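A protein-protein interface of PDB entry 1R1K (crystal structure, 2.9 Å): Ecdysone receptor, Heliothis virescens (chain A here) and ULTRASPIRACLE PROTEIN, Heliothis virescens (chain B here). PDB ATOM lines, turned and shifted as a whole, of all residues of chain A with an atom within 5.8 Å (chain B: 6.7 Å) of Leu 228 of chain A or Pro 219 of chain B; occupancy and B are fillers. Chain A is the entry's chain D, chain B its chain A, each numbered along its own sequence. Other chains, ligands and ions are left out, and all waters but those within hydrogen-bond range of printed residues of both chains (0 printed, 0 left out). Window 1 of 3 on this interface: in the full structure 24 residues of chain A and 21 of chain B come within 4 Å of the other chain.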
ATOM      1  N   GLU A 112      21.079  -1.999  18.878  1.00  0.00           N
ATOM      2  CA  GLU A 112      22.334  -1.646  18.217  1.00  0.00           C
ATOM      3  C   GLU A 112      23.594  -1.879  19.085  1.00  0.00           C
ATOM      4  O   GLU A 112      24.670  -2.185  18.573  1.00  0.00           O
ATOM      5  CB  GLU A 112      22.280  -0.186  17.765  1.00  0.00           C
ATOM      6  CG  GLU A 112      21.265   0.134  16.693  1.00  0.00           C
ATOM      7  CD  GLU A 112      21.380   1.575  16.210  1.00  0.00           C
ATOM      8  OE1 GLU A 112      20.405   2.110  15.639  1.00  0.00           O
ATOM      9  OE2 GLU A 112      22.459   2.189  16.393  1.00  0.00           O
ATOM     10  N   LEU A 174      32.469   4.204  22.051  1.00  0.00           N
ATOM     11  CA  LEU A 174      31.520   3.946  20.968  1.00  0.00           C
ATOM     12  C   LEU A 174      30.127   3.669  21.520  1.00  0.00           C
ATOM     13  O   LEU A 174      29.148   4.311  21.122  1.00  0.00           O
ATOM     14  CB  LEU A 174      31.958   2.742  20.133  1.00  0.00           C
ATOM     15  CG  LEU A 174      31.085   2.457  18.905  1.00  0.00           C
ATOM     16  CD1 LEU A 174      31.117   3.633  17.948  1.00  0.00           C
ATOM     17  CD2 LEU A 174      31.583   1.224  18.214  1.00  0.00           C
ATOM     18  N   ILE A 177      28.371   6.685  22.849  1.00  0.00           N
ATOM     19  CA  ILE A 177      27.965   7.471  21.701  1.00  0.00           C
ATOM     20  C   ILE A 177      26.625   6.986  21.129  1.00  0.00           C
ATOM     21  O   ILE A 177      25.651   7.745  21.090  1.00  0.00           O
ATOM     22  CB  ILE A 177      29.063   7.429  20.638  1.00  0.00           C
ATOM     23  CG1 ILE A 177      30.333   8.058  21.229  1.00  0.00           C
ATOM     24  CG2 ILE A 177      28.587   8.118  19.375  1.00  0.00           C
ATOM     25  CD1 ILE A 177      31.456   8.353  20.248  1.00  0.00           C
ATOM     26  N   VAL A 178      26.585   5.723  20.694  1.00  0.00           N
ATOM     27  CA  VAL A 178      25.366   5.094  20.152  1.00  0.00           C
ATOM     28  C   VAL A 178      24.127   5.475  20.993  1.00  0.00           C
ATOM     29  O   VAL A 178      23.085   5.858  20.456  1.00  0.00           O
ATOM     30  CB  VAL A 178      25.545   3.547  20.126  1.00  0.00           C
ATOM     31  CG1 VAL A 178      24.226   2.829  19.963  1.00  0.00           C
ATOM     32  CG2 VAL A 178      26.468   3.188  19.018  1.00  0.00           C
ATOM     33  N   SER A 181      22.880   8.915  20.501  1.00  0.00           N
ATOM     34  CA  SER A 181      22.753   9.101  19.073  1.00  0.00           C
ATOM     35  C   SER A 181      21.364   9.675  18.875  1.00  0.00           C
ATOM     36  O   SER A 181      20.413   9.217  19.498  1.00  0.00           O
ATOM     37  CB  SER A 181      22.858   7.765  18.358  1.00  0.00           C
ATOM     38  OG  SER A 181      24.163   7.556  17.851  1.00  0.00           O
ATOM     39  N   ILE A 224      35.698   3.958  12.780  1.00  0.00           N
ATOM     40  CA  ILE A 224      34.960   3.729  13.994  1.00  0.00           C
ATOM     41  C   ILE A 224      33.575   4.356  13.877  1.00  0.00           C
ATOM     42  O   ILE A 224      32.561   3.671  14.047  1.00  0.00           O
ATOM     43  CB  ILE A 224      35.751   4.276  15.209  1.00  0.00           C
ATOM     44  CG1 ILE A 224      36.936   3.343  15.486  1.00  0.00           C
ATOM     45  CG2 ILE A 224      34.850   4.418  16.449  1.00  0.00           C
ATOM     46  CD1 ILE A 224      37.543   3.515  16.877  1.00  0.00           C
ATOM     47  N   LEU A 225      33.502   5.640  13.565  1.00  0.00           N
ATOM     48  CA  LEU A 225      32.190   6.262  13.432  1.00  0.00           C
ATOM     49  C   LEU A 225      31.324   5.541  12.370  1.00  0.00           C
ATOM     50  O   LEU A 225      30.099   5.645  12.380  1.00  0.00           O
ATOM     51  CB  LEU A 225      32.340   7.763  13.101  1.00  0.00           C
ATOM     52  CG  LEU A 225      32.748   8.658  14.291  1.00  0.00           C
ATOM     53  CD1 LEU A 225      32.259  10.048  14.077  1.00  0.00           C
ATOM     54  CD2 LEU A 225      32.132   8.154  15.584  1.00  0.00           C
ATOM     55  N   GLY A 226      31.981   4.806  11.466  1.00  0.00           N
ATOM     56  CA  GLY A 226      31.315   4.068  10.404  1.00  0.00           C
ATOM     57  C   GLY A 226      30.545   2.925  10.985  1.00  0.00           C
ATOM     58  O   GLY A 226      29.531   2.536  10.440  1.00  0.00           O
ATOM     59  N   ILE A 227      31.032   2.370  12.085  1.00  0.00           N
ATOM     60  CA  ILE A 227      30.337   1.286  12.756  1.00  0.00           C
ATOM     61  C   ILE A 227      28.881   1.732  13.048  1.00  0.00           C
ATOM     62  O   ILE A 227      27.932   0.924  13.065  1.00  0.00           O
ATOM     63  CB  ILE A 227      31.021   0.953  14.096  1.00  0.00           C
ATOM     64  CG1 ILE A 227      32.417   0.360  13.816  1.00  0.00           C
ATOM     65  CG2 ILE A 227      30.069   0.073  14.973  1.00  0.00           C
ATOM     66  CD1 ILE A 227      33.347   0.298  15.057  1.00  0.00           C
ATOM     67  N   LEU A 228      28.708   3.022  13.288  1.00  0.00           N
ATOM     68  CA  LEU A 228      27.386   3.510  13.548  1.00  0.00           C
ATOM     69  C   LEU A 228      26.428   3.120  12.421  1.00  0.00           C
ATOM     70  O   LEU A 228      25.401   2.482  12.656  1.00  0.00           O
ATOM     71  CB  LEU A 228      27.395   5.023  13.687  1.00  0.00           C
ATOM     72  CG  LEU A 228      28.168   5.574  14.863  1.00  0.00           C
ATOM     73  CD1 LEU A 228      27.970   7.041  14.856  1.00  0.00           C
ATOM     74  CD2 LEU A 228      27.730   4.937  16.165  1.00  0.00           C
ATOM     75  N   THR A 229      26.746   3.470  11.187  1.00  0.00           N
ATOM     76  CA  THR A 229      25.792   3.148  10.153  1.00  0.00           C
ATOM     77  C   THR A 229      25.555   1.639   9.929  1.00  0.00           C
ATOM     78  O   THR A 229      24.457   1.209   9.645  1.00  0.00           O
ATOM     79  CB  THR A 229      26.125   3.924   8.842  1.00  0.00           C
ATOM     80  OG1 THR A 229      26.209   3.013   7.750  1.00  0.00           O
ATOM     81  CG2 THR A 229      27.396   4.717   8.981  1.00  0.00           C
ATOM     82  N   GLU A 230      26.564   0.816  10.090  1.00  0.00           N
ATOM     83  CA  GLU A 230      26.319  -0.611   9.890  1.00  0.00           C
ATOM     84  C   GLU A 230      25.368  -1.166  10.975  1.00  0.00           C
ATOM     85  O   GLU A 230      24.506  -2.030  10.737  1.00  0.00           O
ATOM     86  CB  GLU A 230      27.653  -1.355   9.907  1.00  0.00           C
ATOM     87  CG  GLU A 230      28.456  -1.001   8.718  1.00  0.00           C
ATOM     88  CD  GLU A 230      27.665  -1.253   7.470  1.00  0.00           C
ATOM     89  OE1 GLU A 230      27.166  -2.386   7.348  1.00  0.00           O
ATOM     90  OE2 GLU A 230      27.526  -0.341   6.625  1.00  0.00           O
ATOM     91  N   ILE A 231      25.558  -0.649  12.178  1.00  0.00           N
ATOM     92  CA  ILE A 231      24.781  -1.035  13.320  1.00  0.00           C
ATOM     93  C   ILE A 231      23.290  -0.670  13.118  1.00  0.00           C
ATOM     94  O   ILE A 231      22.405  -1.253  13.734  1.00  0.00           O
ATOM     95  CB  ILE A 231      25.478  -0.386  14.535  1.00  0.00           C
ATOM     96  CG1 ILE A 231      26.637  -1.264  14.889  1.00  0.00           C
ATOM     97  CG2 ILE A 231      24.583  -0.190  15.725  1.00  0.00           C
ATOM     98  CD1 ILE A 231      26.261  -2.696  15.005  1.00  0.00           C
ATOM     99  N   ARG A 232      23.019   0.286  12.236  1.00  0.00           N
ATOM    100  CA  ARG A 232      21.641   0.677  11.936  1.00  0.00           C
ATOM    101  C   ARG A 232      20.997  -0.407  11.036  1.00  0.00           C
ATOM    102  O   ARG A 232      19.819  -0.757  11.206  1.00  0.00           O
ATOM    103  CB  ARG A 232      21.609   2.031  11.231  1.00  0.00           C
ATOM    104  CG  ARG A 232      22.219   3.131  12.046  1.00  0.00           C
ATOM    105  CD  ARG A 232      21.415   3.375  13.344  1.00  0.00           C
ATOM    106  NE  ARG A 232      20.473   4.477  13.193  1.00  0.00           N
ATOM    107  CZ  ARG A 232      20.777   5.743  13.408  1.00  0.00           C
ATOM    108  NH1 ARG A 232      21.992   6.071  13.804  1.00  0.00           N
ATOM    109  NH2 ARG A 232      19.871   6.674  13.176  1.00  0.00           N
ATOM    110  N   THR A 233      21.757  -0.949  10.090  1.00  0.00           N
ATOM    111  CA  THR A 233      21.216  -1.993   9.253  1.00  0.00           C
ATOM    112  C   THR A 233      20.949  -3.297  10.027  1.00  0.00           C
ATOM    113  O   THR A 233      19.958  -3.980   9.764  1.00  0.00           O
ATOM    114  CB  THR A 233      22.147  -2.305   8.102  1.00  0.00           C
ATOM    115  OG1 THR A 233      22.107  -1.218   7.160  1.00  0.00           O
ATOM    116  CG2 THR A 233      21.755  -3.638   7.448  1.00  0.00           C
ATOM    117  N   GLU B  85      20.653   5.173  -0.894  1.00  0.00           N
ATOM    118  CA  GLU B  85      21.296   6.124   0.007  1.00  0.00           C
ATOM    119  C   GLU B  85      21.765   7.342  -0.773  1.00  0.00           C
ATOM    120  O   GLU B  85      21.531   8.499  -0.370  1.00  0.00           O
ATOM    121  CB  GLU B  85      22.482   5.455   0.694  1.00  0.00           C
ATOM    122  CG  GLU B  85      22.357   5.309   2.190  1.00  0.00           C
ATOM    123  CD  GLU B  85      23.097   4.080   2.718  1.00  0.00           C
ATOM    124  OE1 GLU B  85      23.290   3.982   3.949  1.00  0.00           O
ATOM    125  OE2 GLU B  85      23.472   3.198   1.908  1.00  0.00           O
ATOM    126  N   ARG B 144      11.522  12.542   8.075  1.00  0.00           N
ATOM    127  CA  ARG B 144      12.861  12.224   8.518  1.00  0.00           C
ATOM    128  C   ARG B 144      13.883  12.754   7.507  1.00  0.00           C
ATOM    129  O   ARG B 144      14.890  13.345   7.883  1.00  0.00           O
ATOM    130  CB  ARG B 144      12.984  10.718   8.769  1.00  0.00           C
ATOM    131  CG  ARG B 144      12.425  10.359  10.168  1.00  0.00           C
ATOM    132  CD  ARG B 144      12.381   8.869  10.484  1.00  0.00           C
ATOM    133  NE  ARG B 144      13.686   8.285  10.775  1.00  0.00           N
ATOM    134  CZ  ARG B 144      13.935   6.983  10.645  1.00  0.00           C
ATOM    135  NH1 ARG B 144      12.950   6.190  10.218  1.00  0.00           N
ATOM    136  NH2 ARG B 144      15.135   6.461  10.958  1.00  0.00           N
ATOM    137  N   GLU B 148      16.268  15.179   9.750  1.00  0.00           N
ATOM    138  CA  GLU B 148      17.560  14.566  10.022  1.00  0.00           C
ATOM    139  C   GLU B 148      18.593  14.852   8.950  1.00  0.00           C
ATOM    140  O   GLU B 148      19.778  14.905   9.247  1.00  0.00           O
ATOM    141  CB  GLU B 148      17.418  13.056  10.154  1.00  0.00           C
ATOM    142  CG  GLU B 148      16.490  12.629  11.245  1.00  0.00           C
ATOM    143  CD  GLU B 148      16.231  11.136  11.244  1.00  0.00           C
ATOM    144  OE1 GLU B 148      15.279  10.716  11.927  1.00  0.00           O
ATOM    145  OE2 GLU B 148      16.964  10.380  10.574  1.00  0.00           O
ATOM    146  N   LEU B 214      29.590  15.526  10.374  1.00  0.00           N
ATOM    147  CA  LEU B 214      29.301  15.224   8.976  1.00  0.00           C
ATOM    148  C   LEU B 214      29.151  13.707   8.828  1.00  0.00           C
ATOM    149  O   LEU B 214      28.208  13.205   8.191  1.00  0.00           O
ATOM    150  CB  LEU B 214      30.422  15.708   8.048  1.00  0.00           C
ATOM    151  CG  LEU B 214      30.768  17.193   7.937  1.00  0.00           C
ATOM    152  CD1 LEU B 214      31.868  17.367   6.894  1.00  0.00           C
ATOM    153  CD2 LEU B 214      29.552  17.979   7.536  1.00  0.00           C
ATOM    154  N   LEU B 215      30.085  12.974   9.425  1.00  0.00           N
ATOM    155  CA  LEU B 215      30.051  11.520   9.346  1.00  0.00           C
ATOM    156  C   LEU B 215      28.917  10.903  10.152  1.00  0.00           C
ATOM    157  O   LEU B 215      28.635   9.715  10.008  1.00  0.00           O
ATOM    158  CB  LEU B 215      31.385  10.935   9.798  1.00  0.00           C
ATOM    159  CG  LEU B 215      32.468  11.121   8.745  1.00  0.00           C
ATOM    160  CD1 LEU B 215      33.792  10.541   9.228  1.00  0.00           C
ATOM    161  CD2 LEU B 215      32.032  10.434   7.478  1.00  0.00           C
ATOM    162  N   LEU B 216      28.253  11.713  10.968  1.00  0.00           N
ATOM    163  CA  LEU B 216      27.170  11.235  11.804  1.00  0.00           C
ATOM    164  C   LEU B 216      25.838  11.328  11.081  1.00  0.00           C
ATOM    165  O   LEU B 216      24.779  11.063  11.665  1.00  0.00           O
ATOM    166  CB  LEU B 216      27.127  12.059  13.082  1.00  0.00           C
ATOM    167  CG  LEU B 216      26.935  11.334  14.407  1.00  0.00           C
ATOM    168  CD1 LEU B 216      27.894  10.198  14.496  1.00  0.00           C
ATOM    169  CD2 LEU B 216      27.141  12.309  15.557  1.00  0.00           C
ATOM    170  N   ARG B 217      25.890  11.730   9.811  1.00  0.00           N
ATOM    171  CA  ARG B 217      24.692  11.837   8.968  1.00  0.00           C
ATOM    172  C   ARG B 217      24.546  10.495   8.283  1.00  0.00           C
ATOM    173  O   ARG B 217      23.446  10.056   7.948  1.00  0.00           O
ATOM    174  CB  ARG B 217      24.866  12.912   7.900  1.00  0.00           C
ATOM    175  CG  ARG B 217      24.993  14.303   8.431  1.00  0.00           C
ATOM    176  CD  ARG B 217      23.827  14.602   9.302  1.00  0.00           C
ATOM    177  NE  ARG B 217      24.172  14.547  10.713  1.00  0.00           N
ATOM    178  CZ  ARG B 217      23.291  14.290  11.679  1.00  0.00           C
ATOM    179  NH1 ARG B 217      22.013  14.050  11.367  1.00  0.00           N
ATOM    180  NH2 ARG B 217      23.673  14.307  12.959  1.00  0.00           N
ATOM    181  N   LEU B 218      25.682   9.842   8.087  1.00  0.00           N
ATOM    182  CA  LEU B 218      25.710   8.552   7.447  1.00  0.00           C
ATOM    183  C   LEU B 218      24.791   7.523   8.058  1.00  0.00           C
ATOM    184  O   LEU B 218      24.261   6.697   7.342  1.00  0.00           O
ATOM    185  CB  LEU B 218      27.133   8.018   7.413  1.00  0.00           C
ATOM    186  CG  LEU B 218      28.003   8.566   6.270  1.00  0.00           C
ATOM    187  CD1 LEU B 218      27.165   9.387   5.278  1.00  0.00           C
ATOM    188  CD2 LEU B 218      29.114   9.396   6.865  1.00  0.00           C
ATOM    189  N   PRO B 219      24.615   7.526   9.391  1.00  0.00           N
ATOM    190  CA  PRO B 219      23.708   6.519   9.963  1.00  0.00           C
ATOM    191  C   PRO B 219      22.290   6.989   9.741  1.00  0.00           C
ATOM    192  O   PRO B 219      21.465   6.247   9.226  1.00  0.00           O
ATOM    193  CB  PRO B 219      24.072   6.488  11.450  1.00  0.00           C
ATOM    194  CG  PRO B 219      25.465   7.004  11.489  1.00  0.00           C
ATOM    195  CD  PRO B 219      25.455   8.119  10.443  1.00  0.00           C
ATOM    196  N   ALA B 220      22.014   8.233  10.124  1.00  0.00           N
ATOM    197  CA  ALA B 220      20.683   8.819   9.933  1.00  0.00           C
ATOM    198  C   ALA B 220      20.220   8.536   8.489  1.00  0.00           C
ATOM    199  O   ALA B 220      19.039   8.286   8.229  1.00  0.00           O
ATOM    200  CB  ALA B 220      20.731  10.335  10.199  1.00  0.00           C
ATOM    201  N   LEU B 221      21.169   8.557   7.562  1.00  0.00           N
ATOM    202  CA  LEU B 221      20.859   8.289   6.175  1.00  0.00           C
ATOM    203  C   LEU B 221      20.576   6.814   5.913  1.00  0.00           C
ATOM    204  O   LEU B 221      19.653   6.484   5.190  1.00  0.00           O
ATOM    205  CB  LEU B 221      22.003   8.740   5.274  1.00  0.00           C
ATOM    206  CG  LEU B 221      21.835   8.335   3.812  1.00  0.00           C
ATOM    207  CD1 LEU B 221      20.509   8.859   3.286  1.00  0.00           C
ATOM    208  CD2 LEU B 221      22.994   8.870   2.998  1.00  0.00           C
ATOM    209  N   ARG B 222      21.377   5.932   6.494  1.00  0.00           N
ATOM    210  CA  ARG B 222      21.234   4.500   6.307  1.00  0.00           C
ATOM    211  C   ARG B 222      19.855   4.039   6.766  1.00  0.00           C
ATOM    212  O   ARG B 222      19.189   3.236   6.097  1.00  0.00           O
ATOM    213  CB  ARG B 222      22.341   3.778   7.089  1.00  0.00           C
ATOM    214  CG  ARG B 222      22.097   2.290   7.347  1.00  0.00           C
ATOM    215  CD  ARG B 222      21.995   1.513   6.075  1.00  0.00           C
ATOM    216  NE  ARG B 222      23.232   1.666   5.336  1.00  0.00           N
ATOM    217  CZ  ARG B 222      24.354   1.030   5.640  1.00  0.00           C
ATOM    218  NH1 ARG B 222      24.384   0.187   6.667  1.00  0.00           N
ATOM    219  NH2 ARG B 222      25.451   1.250   4.934  1.00  0.00           N
ATOM    220  N   SER B 223      19.428   4.559   7.908  1.00  0.00           N
ATOM    221  CA  SER B 223      18.134   4.191   8.459  1.00  0.00           C
ATOM    222  C   SER B 223      16.986   4.603   7.548  1.00  0.00           C
ATOM    223  O   SER B 223      16.069   3.805   7.292  1.00  0.00           O
ATOM    224  CB  SER B 223      17.948   4.815   9.841  1.00  0.00           C
ATOM    225  OG  SER B 223      18.728   4.116  10.799  1.00  0.00           O
ATOM    226  N   ILE B 224      17.031   5.847   7.071  1.00  0.00           N
ATOM    227  CA  ILE B 224      16.003   6.350   6.191  1.00  0.00           C
ATOM    228  C   ILE B 224      15.997   5.500   4.950  1.00  0.00           C
ATOM    229  O   ILE B 224      14.951   5.045   4.516  1.00  0.00           O
ATOM    230  CB  ILE B 224      16.265   7.781   5.777  1.00  0.00           C
ATOM    231  CG1 ILE B 224      16.286   8.683   7.011  1.00  0.00           C
ATOM    232  CG2 ILE B 224      15.195   8.231   4.802  1.00  0.00           C
ATOM    233  CD1 ILE B 224      16.937  10.014   6.777  1.00  0.00           C
ATOM    234  N   SER B 225      17.152   5.261   4.360  1.00  0.00           N
ATOM    235  CA  SER B 225      17.149   4.451   3.161  1.00  0.00           C
ATOM    236  C   SER B 225      16.574   3.065   3.471  1.00  0.00           C
ATOM    237  O   SER B 225      15.790   2.519   2.714  1.00  0.00           O
ATOM    238  CB  SER B 225      18.566   4.312   2.609  1.00  0.00           C
ATOM    239  OG  SER B 225      19.367   3.526   3.480  1.00  0.00           O
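NE of Arg 232 of chain A is in salt-bridge range of OE1 of Glu 112 of chain A (3.4 Å).
The guanidinium group (NE) of Arg 222 of chain B lies within salt-bridge range of the side-chain carboxylate (OE1) of Glu 85 of chain B, at 2.7 Å.
The side-chain hydroxyl of Ser 225 of chain B lies within hydrogen-bond range of the backbone carbonyl oxygen of Arg 222 of chain B, at 2.6 Å.
The backbone carbonyl oxygen (O) of Thr 229 of chain A is in hydrogen-bond range of the guanidinium group (NH1) of Arg 222 of chain B, at 3.1 Å.
The side-chain carboxylate of Glu 230 of chain A is in salt-bridge range of the guanidinium group of Arg 222 of chain B (3.1 Å).
NE of Arg 232 of chain A is in hydrogen-bond range of OG of Ser 223 of chain B, 3.0 Å away.
The side-chain hydroxyl (OG1) of Thr 233 of chain A lies within hydrogen-bond range of the guanidinium group (NH1) of Arg 222 of chain B (2.7 Å).
Of the 15 printed residues of chain A, 5 touch a printed residue of chain B.
Hydrophobic or aromatic side chains of chain A within 4 Å of the printed part of chain B: Leu 228.
Of the 15 printed residues of chain B, 6 touch a printed residue of chain A.
Printed residues of chain B that touch a printed residue of chain A: Leu 216, Leu 218, Pro 219, Ala 220, Arg 222 and Ser 223.
Hydrophobic or aromatic side chains of chain B that line the printed part of chain A: Leu 216, Leu 218 and Pro 219.
Among the printed residues, Asp or Glu carboxylates within 4 Å of a Lys or Arg side-chain nitrogen of the other chain: Glu 230 of chain A with Arg 222 of chain B.
Ser 181 of chain A touches none of the printed residues of chain B.
Ile 227 of chain A touches none of the printed residues of chain B.
Printed residues of chain B within 4 Å of Leu 228 of chain A: Leu 216 (3.2 Å) and Pro 219 (3.5 Å).
Of the printed residues of chain B, Thr 229 of chain A touches Leu 218, Pro 219 and Arg 222.
Printed residues of chain B within 4 Å of Arg 232 of chain A: Pro 219 (3.2 Å), Ala 220 (3.97 Å), Arg 222 (3.9 Å) and Ser 223 (3.0 Å).
Printed residues of chain A within 4 Å of Pro 219 of chain B: Leu 228 (3.5 Å), Thr 229 (3.7 Å) and Arg 232 (3.2 Å).
The nearest printed residue of chain B that does not touch Thr 229 of chain A is Glu 85 of chain B (4.9 Å).
Leu 228 of chain A touches Leu 216 of chain B.
CB of Leu 228 of chain A touches CG of Pro 219 of chain B, 3.5 Å away.
O of Leu 218 of chain B touches CB of Thr 229 of chain A (3.7 Å).
Thr 229 of chain A touches Pro 219 of chain B.
NH1 of Arg 232 of chain A touches CB of Pro 219 of chain B, at 3.2 Å.
CA of Ala 220 of chain B touches NH2 of Arg 232 of chain A (3.97 Å).
CG of Arg 222 of chain B touches CB of Arg 232 of chain A, 3.9 Å away.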
